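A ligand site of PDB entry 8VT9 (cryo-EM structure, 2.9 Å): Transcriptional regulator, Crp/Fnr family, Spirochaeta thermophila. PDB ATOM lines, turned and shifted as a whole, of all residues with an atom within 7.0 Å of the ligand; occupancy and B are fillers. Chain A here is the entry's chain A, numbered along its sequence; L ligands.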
ATOM      1  N   ILE A 348     -20.835 -32.605 -12.538  1.00  0.00           N
ATOM      2  CA  ILE A 348     -20.970 -31.366 -13.286  1.00  0.00           C
ATOM      3  C   ILE A 348     -19.837 -30.428 -12.872  1.00  0.00           C
ATOM      4  O   ILE A 348     -19.571 -30.262 -11.671  1.00  0.00           O
ATOM      5  CB  ILE A 348     -22.342 -30.697 -13.061  1.00  0.00           C
ATOM      6  CG1 ILE A 348     -23.443 -31.502 -13.740  1.00  0.00           C
ATOM      7  CG2 ILE A 348     -22.333 -29.255 -13.538  1.00  0.00           C
ATOM      8  CD1 ILE A 348     -24.829 -30.962 -13.482  1.00  0.00           C
ATOM      9  N   ALA A 350     -18.562 -26.431 -13.366  1.00  0.00           N
ATOM     10  CA  ALA A 350     -19.141 -25.147 -13.724  1.00  0.00           C
ATOM     11  C   ALA A 350     -18.474 -24.571 -14.971  1.00  0.00           C
ATOM     12  O   ALA A 350     -17.290 -24.793 -15.227  1.00  0.00           O
ATOM     13  CB  ALA A 350     -19.027 -24.161 -12.575  1.00  0.00           C
ATOM     14  N   GLY A 354     -23.372 -27.824 -20.127  1.00  0.00           N
ATOM     15  CA  GLY A 354     -24.230 -28.863 -19.578  1.00  0.00           C
ATOM     16  C   GLY A 354     -25.447 -29.156 -20.426  1.00  0.00           C
ATOM     17  O   GLY A 354     -26.169 -28.244 -20.830  1.00  0.00           O
ATOM     18  N   ASP A 356     -27.592 -32.239 -19.647  1.00  0.00           N
ATOM     19  CA  ASP A 356     -28.221 -33.440 -19.093  1.00  0.00           C
ATOM     20  C   ASP A 356     -28.742 -33.237 -17.677  1.00  0.00           C
ATOM     21  O   ASP A 356     -27.978 -32.979 -16.742  1.00  0.00           O
ATOM     22  CB  ASP A 356     -27.216 -34.603 -19.117  1.00  0.00           C
ATOM     23  CG  ASP A 356     -25.872 -34.235 -18.522  1.00  0.00           C
ATOM     24  OD1 ASP A 356     -25.622 -33.030 -18.275  1.00  0.00           O
ATOM     25  OD2 ASP A 356     -25.040 -35.155 -18.317  1.00  0.00           O
ATOM     26  N   TYR A 358     -30.363 -34.602 -14.127  1.00  0.00           N
ATOM     27  CA  TYR A 358     -29.992 -35.737 -13.288  1.00  0.00           C
ATOM     28  C   TYR A 358     -31.027 -35.961 -12.203  1.00  0.00           C
ATOM     29  O   TYR A 358     -31.734 -35.035 -11.801  1.00  0.00           O
ATOM     30  CB  TYR A 358     -28.615 -35.538 -12.652  1.00  0.00           C
ATOM     31  CG  TYR A 358     -27.464 -35.640 -13.619  1.00  0.00           C
ATOM     32  CD1 TYR A 358     -26.940 -36.865 -13.981  1.00  0.00           C
ATOM     33  CD2 TYR A 358     -26.898 -34.490 -14.165  1.00  0.00           C
ATOM     34  CE1 TYR A 358     -25.884 -36.956 -14.855  1.00  0.00           C
ATOM     35  CE2 TYR A 358     -25.839 -34.575 -15.052  1.00  0.00           C
ATOM     36  CZ  TYR A 358     -25.343 -35.819 -15.388  1.00  0.00           C
ATOM     37  OH  TYR A 358     -24.289 -35.917 -16.274  1.00  0.00           O
ATOM     38  N   VAL A 367     -23.401 -29.861  -4.148  1.00  0.00           N
ATOM     39  CA  VAL A 367     -23.330 -28.772  -5.105  1.00  0.00           C
ATOM     40  C   VAL A 367     -22.383 -27.724  -4.544  1.00  0.00           C
ATOM     41  O   VAL A 367     -22.634 -27.178  -3.455  1.00  0.00           O
ATOM     42  CB  VAL A 367     -24.715 -28.169  -5.384  1.00  0.00           C
ATOM     43  CG1 VAL A 367     -24.618 -27.038  -6.388  1.00  0.00           C
ATOM     44  CG2 VAL A 367     -25.678 -29.243  -5.858  1.00  0.00           C
ATOM     45  N   LEU A 368     -21.305 -27.452  -5.279  1.00  0.00           N
ATOM     46  CA  LEU A 368     -20.208 -26.590  -4.853  1.00  0.00           C
ATOM     47  C   LEU A 368     -20.038 -25.440  -5.823  1.00  0.00           C
ATOM     48  O   LEU A 368     -20.398 -25.539  -7.000  1.00  0.00           O
ATOM     49  CB  LEU A 368     -18.888 -27.368  -4.758  1.00  0.00           C
ATOM     50  CG  LEU A 368     -18.478 -28.210  -3.537  1.00  0.00           C
ATOM     51  CD1 LEU A 368     -17.967 -27.323  -2.407  1.00  0.00           C
ATOM     52  CD2 LEU A 368     -19.610 -29.087  -3.053  1.00  0.00           C
ATOM     53  N   TYR A 376     -22.642 -25.092  -1.991  1.00  0.00           N
ATOM     54  CA  TYR A 376     -23.970 -24.512  -2.155  1.00  0.00           C
ATOM     55  C   TYR A 376     -25.038 -25.367  -1.502  1.00  0.00           C
ATOM     56  O   TYR A 376     -25.934 -24.841  -0.835  1.00  0.00           O
ATOM     57  CB  TYR A 376     -24.288 -24.332  -3.640  1.00  0.00           C
ATOM     58  CG  TYR A 376     -23.496 -23.245  -4.318  1.00  0.00           C
ATOM     59  CD1 TYR A 376     -22.743 -22.333  -3.572  1.00  0.00           C
ATOM     60  CD2 TYR A 376     -23.510 -23.106  -5.693  1.00  0.00           C
ATOM     61  CE1 TYR A 376     -22.018 -21.331  -4.194  1.00  0.00           C
ATOM     62  CE2 TYR A 376     -22.803 -22.106  -6.328  1.00  0.00           C
ATOM     63  CZ  TYR A 376     -22.058 -21.229  -5.576  1.00  0.00           C
ATOM     64  OH  TYR A 376     -21.340 -20.232  -6.202  1.00  0.00           O
ATOM     65  N   ALA A 377     -24.965 -26.684  -1.665  1.00  0.00           N
ATOM     66  CA  ALA A 377     -26.060 -27.530  -1.190  1.00  0.00           C
ATOM     67  C   ALA A 377     -25.597 -28.964  -1.048  1.00  0.00           C
ATOM     68  O   ALA A 377     -24.571 -29.367  -1.594  1.00  0.00           O
ATOM     69  CB  ALA A 377     -27.268 -27.453  -2.128  1.00  0.00           C
ATOM     70  N   ILE A 378     -26.369 -29.737  -0.292  1.00  0.00           N
ATOM     71  CA  ILE A 378     -26.254 -31.194  -0.247  1.00  0.00           C
ATOM     72  C   ILE A 378     -27.594 -31.782  -0.662  1.00  0.00           C
ATOM     73  O   ILE A 378     -28.641 -31.415  -0.105  1.00  0.00           O
ATOM     74  CB  ILE A 378     -25.834 -31.683   1.147  1.00  0.00           C
ATOM     75  CG1 ILE A 378     -25.993 -33.199   1.265  1.00  0.00           C
ATOM     76  CG2 ILE A 378     -26.618 -30.957   2.243  1.00  0.00           C
ATOM     77  CD1 ILE A 378     -24.957 -33.997   0.485  1.00  0.00           C
ATOM     78  N   LEU A 379     -27.577 -32.665  -1.644  1.00  0.00           N
ATOM     79  CA  LEU A 379     -28.775 -33.319  -2.150  1.00  0.00           C
ATOM     80  C   LEU A 379     -28.648 -34.825  -1.925  1.00  0.00           C
ATOM     81  O   LEU A 379     -27.550 -35.370  -1.905  1.00  0.00           O
ATOM     82  CB  LEU A 379     -28.979 -33.031  -3.638  1.00  0.00           C
ATOM     83  CG  LEU A 379     -28.761 -31.584  -4.077  1.00  0.00           C
ATOM     84  CD1 LEU A 379     -28.865 -31.449  -5.595  1.00  0.00           C
ATOM     85  CD2 LEU A 379     -29.756 -30.663  -3.397  1.00  0.00           C
ATOM     86  N   GLN A 383     -33.760 -36.476  -4.781  1.00  0.00           N
ATOM     87  CA  GLN A 383     -33.535 -35.116  -5.251  1.00  0.00           C
ATOM     88  C   GLN A 383     -32.979 -35.128  -6.666  1.00  0.00           C
ATOM     89  O   GLN A 383     -32.570 -36.167  -7.201  1.00  0.00           O
ATOM     90  CB  GLN A 383     -32.592 -34.380  -4.291  1.00  0.00           C
ATOM     91  CG  GLN A 383     -32.730 -32.858  -4.297  1.00  0.00           C
ATOM     92  CD  GLN A 383     -34.065 -32.391  -3.757  1.00  0.00           C
ATOM     93  OE1 GLN A 383     -34.816 -33.148  -3.133  1.00  0.00           O
ATOM     94  NE2 GLN A 383     -34.387 -31.122  -3.996  1.00  0.00           N
ATOM     95  N   PHE A 384     -32.967 -33.954  -7.296  1.00  0.00           N
ATOM     96  CA  PHE A 384     -32.561 -33.817  -8.680  1.00  0.00           C
ATOM     97  C   PHE A 384     -31.802 -32.508  -8.850  1.00  0.00           C
ATOM     98  O   PHE A 384     -31.886 -31.600  -8.016  1.00  0.00           O
ATOM     99  CB  PHE A 384     -33.764 -33.863  -9.626  1.00  0.00           C
ATOM    100  CG  PHE A 384     -34.673 -32.684  -9.484  1.00  0.00           C
ATOM    101  CD1 PHE A 384     -35.593 -32.630  -8.458  1.00  0.00           C
ATOM    102  CD2 PHE A 384     -34.606 -31.627 -10.370  1.00  0.00           C
ATOM    103  CE1 PHE A 384     -36.426 -31.548  -8.318  1.00  0.00           C
ATOM    104  CE2 PHE A 384     -35.434 -30.548 -10.238  1.00  0.00           C
ATOM    105  CZ  PHE A 384     -36.351 -30.502  -9.207  1.00  0.00           C
ATOM    106  N   PHE A 385     -31.052 -32.419  -9.948  1.00  0.00           N
ATOM    107  CA  PHE A 385     -30.296 -31.216 -10.279  1.00  0.00           C
ATOM    108  C   PHE A 385     -30.040 -31.202 -11.772  1.00  0.00           C
ATOM    109  O   PHE A 385     -30.289 -32.182 -12.481  1.00  0.00           O
ATOM    110  CB  PHE A 385     -28.982 -31.152  -9.489  1.00  0.00           C
ATOM    111  CG  PHE A 385     -28.086 -32.330  -9.705  1.00  0.00           C
ATOM    112  CD1 PHE A 385     -28.200 -33.466  -8.930  1.00  0.00           C
ATOM    113  CD2 PHE A 385     -27.112 -32.297 -10.694  1.00  0.00           C
ATOM    114  CE1 PHE A 385     -27.374 -34.547  -9.128  1.00  0.00           C
ATOM    115  CE2 PHE A 385     -26.280 -33.381 -10.899  1.00  0.00           C
ATOM    116  CZ  PHE A 385     -26.405 -34.512 -10.109  1.00  0.00           C
ATOM    117  N   GLY A 386     -29.530 -30.073 -12.261  1.00  0.00           N
ATOM    118  CA  GLY A 386     -29.286 -29.914 -13.682  1.00  0.00           C
ATOM    119  C   GLY A 386     -30.496 -29.542 -14.502  1.00  0.00           C
ATOM    120  O   GLY A 386     -30.466 -29.701 -15.731  1.00  0.00           O
ATOM    121  N   GLU A 387     -31.573 -29.062 -13.877  1.00  0.00           N
ATOM    122  CA  GLU A 387     -32.784 -28.708 -14.602  1.00  0.00           C
ATOM    123  C   GLU A 387     -32.551 -27.655 -15.672  1.00  0.00           C
ATOM    124  O   GLU A 387     -33.185 -27.688 -16.728  1.00  0.00           O
ATOM    125  CB  GLU A 387     -33.850 -28.228 -13.608  1.00  0.00           C
ATOM    126  CG  GLU A 387     -33.329 -27.193 -12.623  1.00  0.00           C
ATOM    127  CD  GLU A 387     -34.310 -26.906 -11.513  1.00  0.00           C
ATOM    128  OE1 GLU A 387     -35.508 -27.218 -11.695  1.00  0.00           O
ATOM    129  OE2 GLU A 387     -33.890 -26.390 -10.456  1.00  0.00           O
ATOM    130  N   MET A 388     -31.615 -26.733 -15.426  1.00  0.00           N
ATOM    131  CA  MET A 388     -31.459 -25.565 -16.295  1.00  0.00           C
ATOM    132  C   MET A 388     -31.158 -25.981 -17.727  1.00  0.00           C
ATOM    133  O   MET A 388     -31.678 -25.379 -18.678  1.00  0.00           O
ATOM    134  CB  MET A 388     -30.363 -24.652 -15.759  1.00  0.00           C
ATOM    135  CG  MET A 388     -30.499 -24.333 -14.275  1.00  0.00           C
ATOM    136  SD  MET A 388     -32.080 -23.574 -13.861  1.00  0.00           S
ATOM    137  CE  MET A 388     -31.997 -22.057 -14.811  1.00  0.00           C
ATOM    138  N   ALA A 389     -30.335 -27.015 -17.903  1.00  0.00           N
ATOM    139  CA  ALA A 389     -29.944 -27.438 -19.252  1.00  0.00           C
ATOM    140  C   ALA A 389     -31.149 -27.856 -20.074  1.00  0.00           C
ATOM    141  O   ALA A 389     -31.105 -27.801 -21.313  1.00  0.00           O
ATOM    142  CB  ALA A 389     -28.935 -28.583 -19.162  1.00  0.00           C
ATOM    143  N   ALA A 394     -27.661 -22.266 -21.493  1.00  0.00           N
ATOM    144  CA  ALA A 394     -26.665 -21.544 -20.735  1.00  0.00           C
ATOM    145  C   ALA A 394     -25.658 -22.508 -20.100  1.00  0.00           C
ATOM    146  O   ALA A 394     -25.994 -23.652 -19.799  1.00  0.00           O
ATOM    147  CB  ALA A 394     -27.337 -20.702 -19.645  1.00  0.00           C
ATOM    148  N   PRO A 395     -24.421 -22.075 -19.917  1.00  0.00           N
ATOM    149  CA  PRO A 395     -23.423 -22.927 -19.250  1.00  0.00           C
ATOM    150  C   PRO A 395     -23.828 -23.214 -17.815  1.00  0.00           C
ATOM    151  O   PRO A 395     -24.650 -22.521 -17.213  1.00  0.00           O
ATOM    152  CB  PRO A 395     -22.140 -22.092 -19.309  1.00  0.00           C
ATOM    153  CG  PRO A 395     -22.592 -20.690 -19.535  1.00  0.00           C
ATOM    154  CD  PRO A 395     -23.828 -20.801 -20.367  1.00  0.00           C
ATOM    155  N   ARG A 396     -23.244 -24.286 -17.278  1.00  0.00           N
ATOM    156  CA  ARG A 396     -23.571 -24.728 -15.927  1.00  0.00           C
ATOM    157  C   ARG A 396     -23.302 -23.634 -14.905  1.00  0.00           C
ATOM    158  O   ARG A 396     -22.295 -22.915 -14.990  1.00  0.00           O
ATOM    159  CB  ARG A 396     -22.771 -25.984 -15.581  1.00  0.00           C
ATOM    160  CG  ARG A 396     -23.120 -27.204 -16.401  1.00  0.00           C
ATOM    161  CD  ARG A 396     -24.514 -27.725 -16.090  1.00  0.00           C
ATOM    162  NE  ARG A 396     -24.659 -29.122 -16.479  1.00  0.00           N
ATOM    163  CZ  ARG A 396     -25.815 -29.763 -16.570  1.00  0.00           C
ATOM    164  NH1 ARG A 396     -26.966 -29.167 -16.284  1.00  0.00           N
ATOM    165  NH2 ARG A 396     -25.822 -31.037 -16.949  1.00  0.00           N
ATOM    166  N   THR A 397     -24.213 -23.502 -13.937  1.00  0.00           N
ATOM    167  CA  THR A 397     -24.084 -22.468 -12.921  1.00  0.00           C
ATOM    168  C   THR A 397     -23.145 -22.842 -11.786  1.00  0.00           C
ATOM    169  O   THR A 397     -22.538 -21.951 -11.181  1.00  0.00           O
ATOM    170  CB  THR A 397     -25.468 -22.139 -12.345  1.00  0.00           C
ATOM    171  OG1 THR A 397     -26.026 -23.313 -11.761  1.00  0.00           O
ATOM    172  CG2 THR A 397     -26.390 -21.634 -13.448  1.00  0.00           C
ATOM    173  N   ALA A 398     -22.997 -24.133 -11.489  1.00  0.00           N
ATOM    174  CA  ALA A 398     -22.172 -24.547 -10.360  1.00  0.00           C
ATOM    175  C   ALA A 398     -21.679 -25.972 -10.574  1.00  0.00           C
ATOM    176  O   ALA A 398     -22.188 -26.702 -11.431  1.00  0.00           O
ATOM    177  CB  ALA A 398     -22.943 -24.465  -9.038  1.00  0.00           C
ATOM    178  N   THR A 399     -20.673 -26.352  -9.799  1.00  0.00           N
ATOM    179  CA  THR A 399     -20.137 -27.703  -9.865  1.00  0.00           C
ATOM    180  C   THR A 399     -20.973 -28.659  -9.018  1.00  0.00           C
ATOM    181  O   THR A 399     -21.565 -28.261  -8.016  1.00  0.00           O
ATOM    182  CB  THR A 399     -18.683 -27.739  -9.388  1.00  0.00           C
ATOM    183  OG1 THR A 399     -18.624 -27.409  -7.995  1.00  0.00           O
ATOM    184  CG2 THR A 399     -17.844 -26.727 -10.161  1.00  0.00           C
ATOM    185  N   VAL A 400     -21.019 -29.914  -9.444  1.00  0.00           N
ATOM    186  CA  VAL A 400     -21.732 -30.961  -8.721  1.00  0.00           C
ATOM    187  C   VAL A 400     -20.792 -32.152  -8.589  1.00  0.00           C
ATOM    188  O   VAL A 400     -20.268 -32.646  -9.596  1.00  0.00           O
ATOM    189  CB  VAL A 400     -23.037 -31.365  -9.442  1.00  0.00           C
ATOM    190  CG1 VAL A 400     -23.866 -32.261  -8.558  1.00  0.00           C
ATOM    191  CG2 VAL A 400     -23.836 -30.136  -9.856  1.00  0.00           C
HETATM  192  P1  LIG L   1     -26.879 -26.445 -13.271  1.00  0.00           P
HETATM  193  O1  LIG L   1     -27.151 -25.370 -14.247  1.00  0.00           O
HETATM  194  O2  LIG L   1     -26.587 -27.786 -13.766  1.00  0.00           O
HETATM  195  O3  LIG L   1     -25.677 -26.013 -12.339  1.00  0.00           O
HETATM  196  C1  LIG L   1     -25.341 -26.909 -11.233  1.00  0.00           C
HETATM  197  C2  LIG L   1     -26.605 -27.161 -10.463  1.00  0.00           C
HETATM  198  O4  LIG L   1     -26.488 -26.876  -9.076  1.00  0.00           O
HETATM  199  C3  LIG L   1     -27.672 -26.187 -10.900  1.00  0.00           C
HETATM  200  O5  LIG L   1     -28.103 -26.509 -12.238  1.00  0.00           O
HETATM  201  C4  LIG L   1     -28.680 -26.382  -9.779  1.00  0.00           C
HETATM  202  O6  LIG L   1     -29.563 -27.475 -10.018  1.00  0.00           O
HETATM  203  C5  LIG L   1     -27.799 -26.700  -8.576  1.00  0.00           C
HETATM  204  N1  LIG L   1     -27.769 -25.623  -7.597  1.00  0.00           N
HETATM  205  C6  LIG L   1     -27.143 -24.413  -7.718  1.00  0.00           C
HETATM  206  N2  LIG L   1     -27.271 -23.643  -6.663  1.00  0.00           N
HETATM  207  C7  LIG L   1     -28.023 -24.417  -5.776  1.00  0.00           C
HETATM  208  C8  LIG L   1     -28.487 -24.165  -4.475  1.00  0.00           C
HETATM  209  N3  LIG L   1     -28.269 -23.032  -3.815  1.00  0.00           N
HETATM  210  N4  LIG L   1     -29.198 -25.151  -3.874  1.00  0.00           N
HETATM  211  C9  LIG L   1     -29.418 -26.292  -4.547  1.00  0.00           C
HETATM  212  N5  LIG L   1     -29.022 -26.627  -5.767  1.00  0.00           N
HETATM  213  C10 LIG L   1     -28.325 -25.641  -6.339  1.00  0.00           C
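The backbone NH of Gly 386 lies within hydrogen-bond range of an oxygen (O6) of the ligand, 3.4 Å away.
The backbone NH (N) of Ala 398 lies within hydrogen-bond range of an oxygen (O3) of the ligand, at 3.4 Å.
An oxygen (O3) of the ligand sits at hydrogen-bond distance from the side-chain hydroxyl (OG1) of Thr 397 (2.8 Å).
The guanidinium group (NH1) of Arg 396 is in salt-bridge range of an oxygen (O2) of the ligand (2.9 Å).
N of Thr 397 is in hydrogen-bond range of O3 of the ligand (3.3 Å).
Ile 348 touches the ligand (CD1 to O2, 3.6 Å).
Val 367 touches the ligand.
Tyr 376 touches the ligand.
Ala 377 touches the ligand.
Phe 385 touches the ligand.
Met 388 touches the ligand.
CG2 of Val 400 touches C1 of the ligand (3.8 Å).
Hydrophobic or aromatic side chains within 4 Å of the ligand: Ile 348, Val 367, Tyr 376, Ala 377, Phe 385, Met 388 and Val 400.
The nearest printed residue that does not touch the ligand is Glu 387 (4.5 Å).
The backbone NH (N) of Tyr 358 sits at hydrogen-bond distance from the backbone carbonyl oxygen (O) of Phe 385 (2.9 Å).
The backbone NH (N) of Val 400 is in hydrogen-bond range of the backbone carbonyl oxygen (O) of Ile 348, 2.7 Å away.
The backbone carbonyl oxygen of Ala 377 lies within hydrogen-bond range of the backbone NH of Val 367.
NH2 of Arg 396 lies within salt-bridge range of OD1 of Asp 356, at 2.4 Å.
N of Tyr 376 is in hydrogen-bond range of O of Val 367 (2.5 Å).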
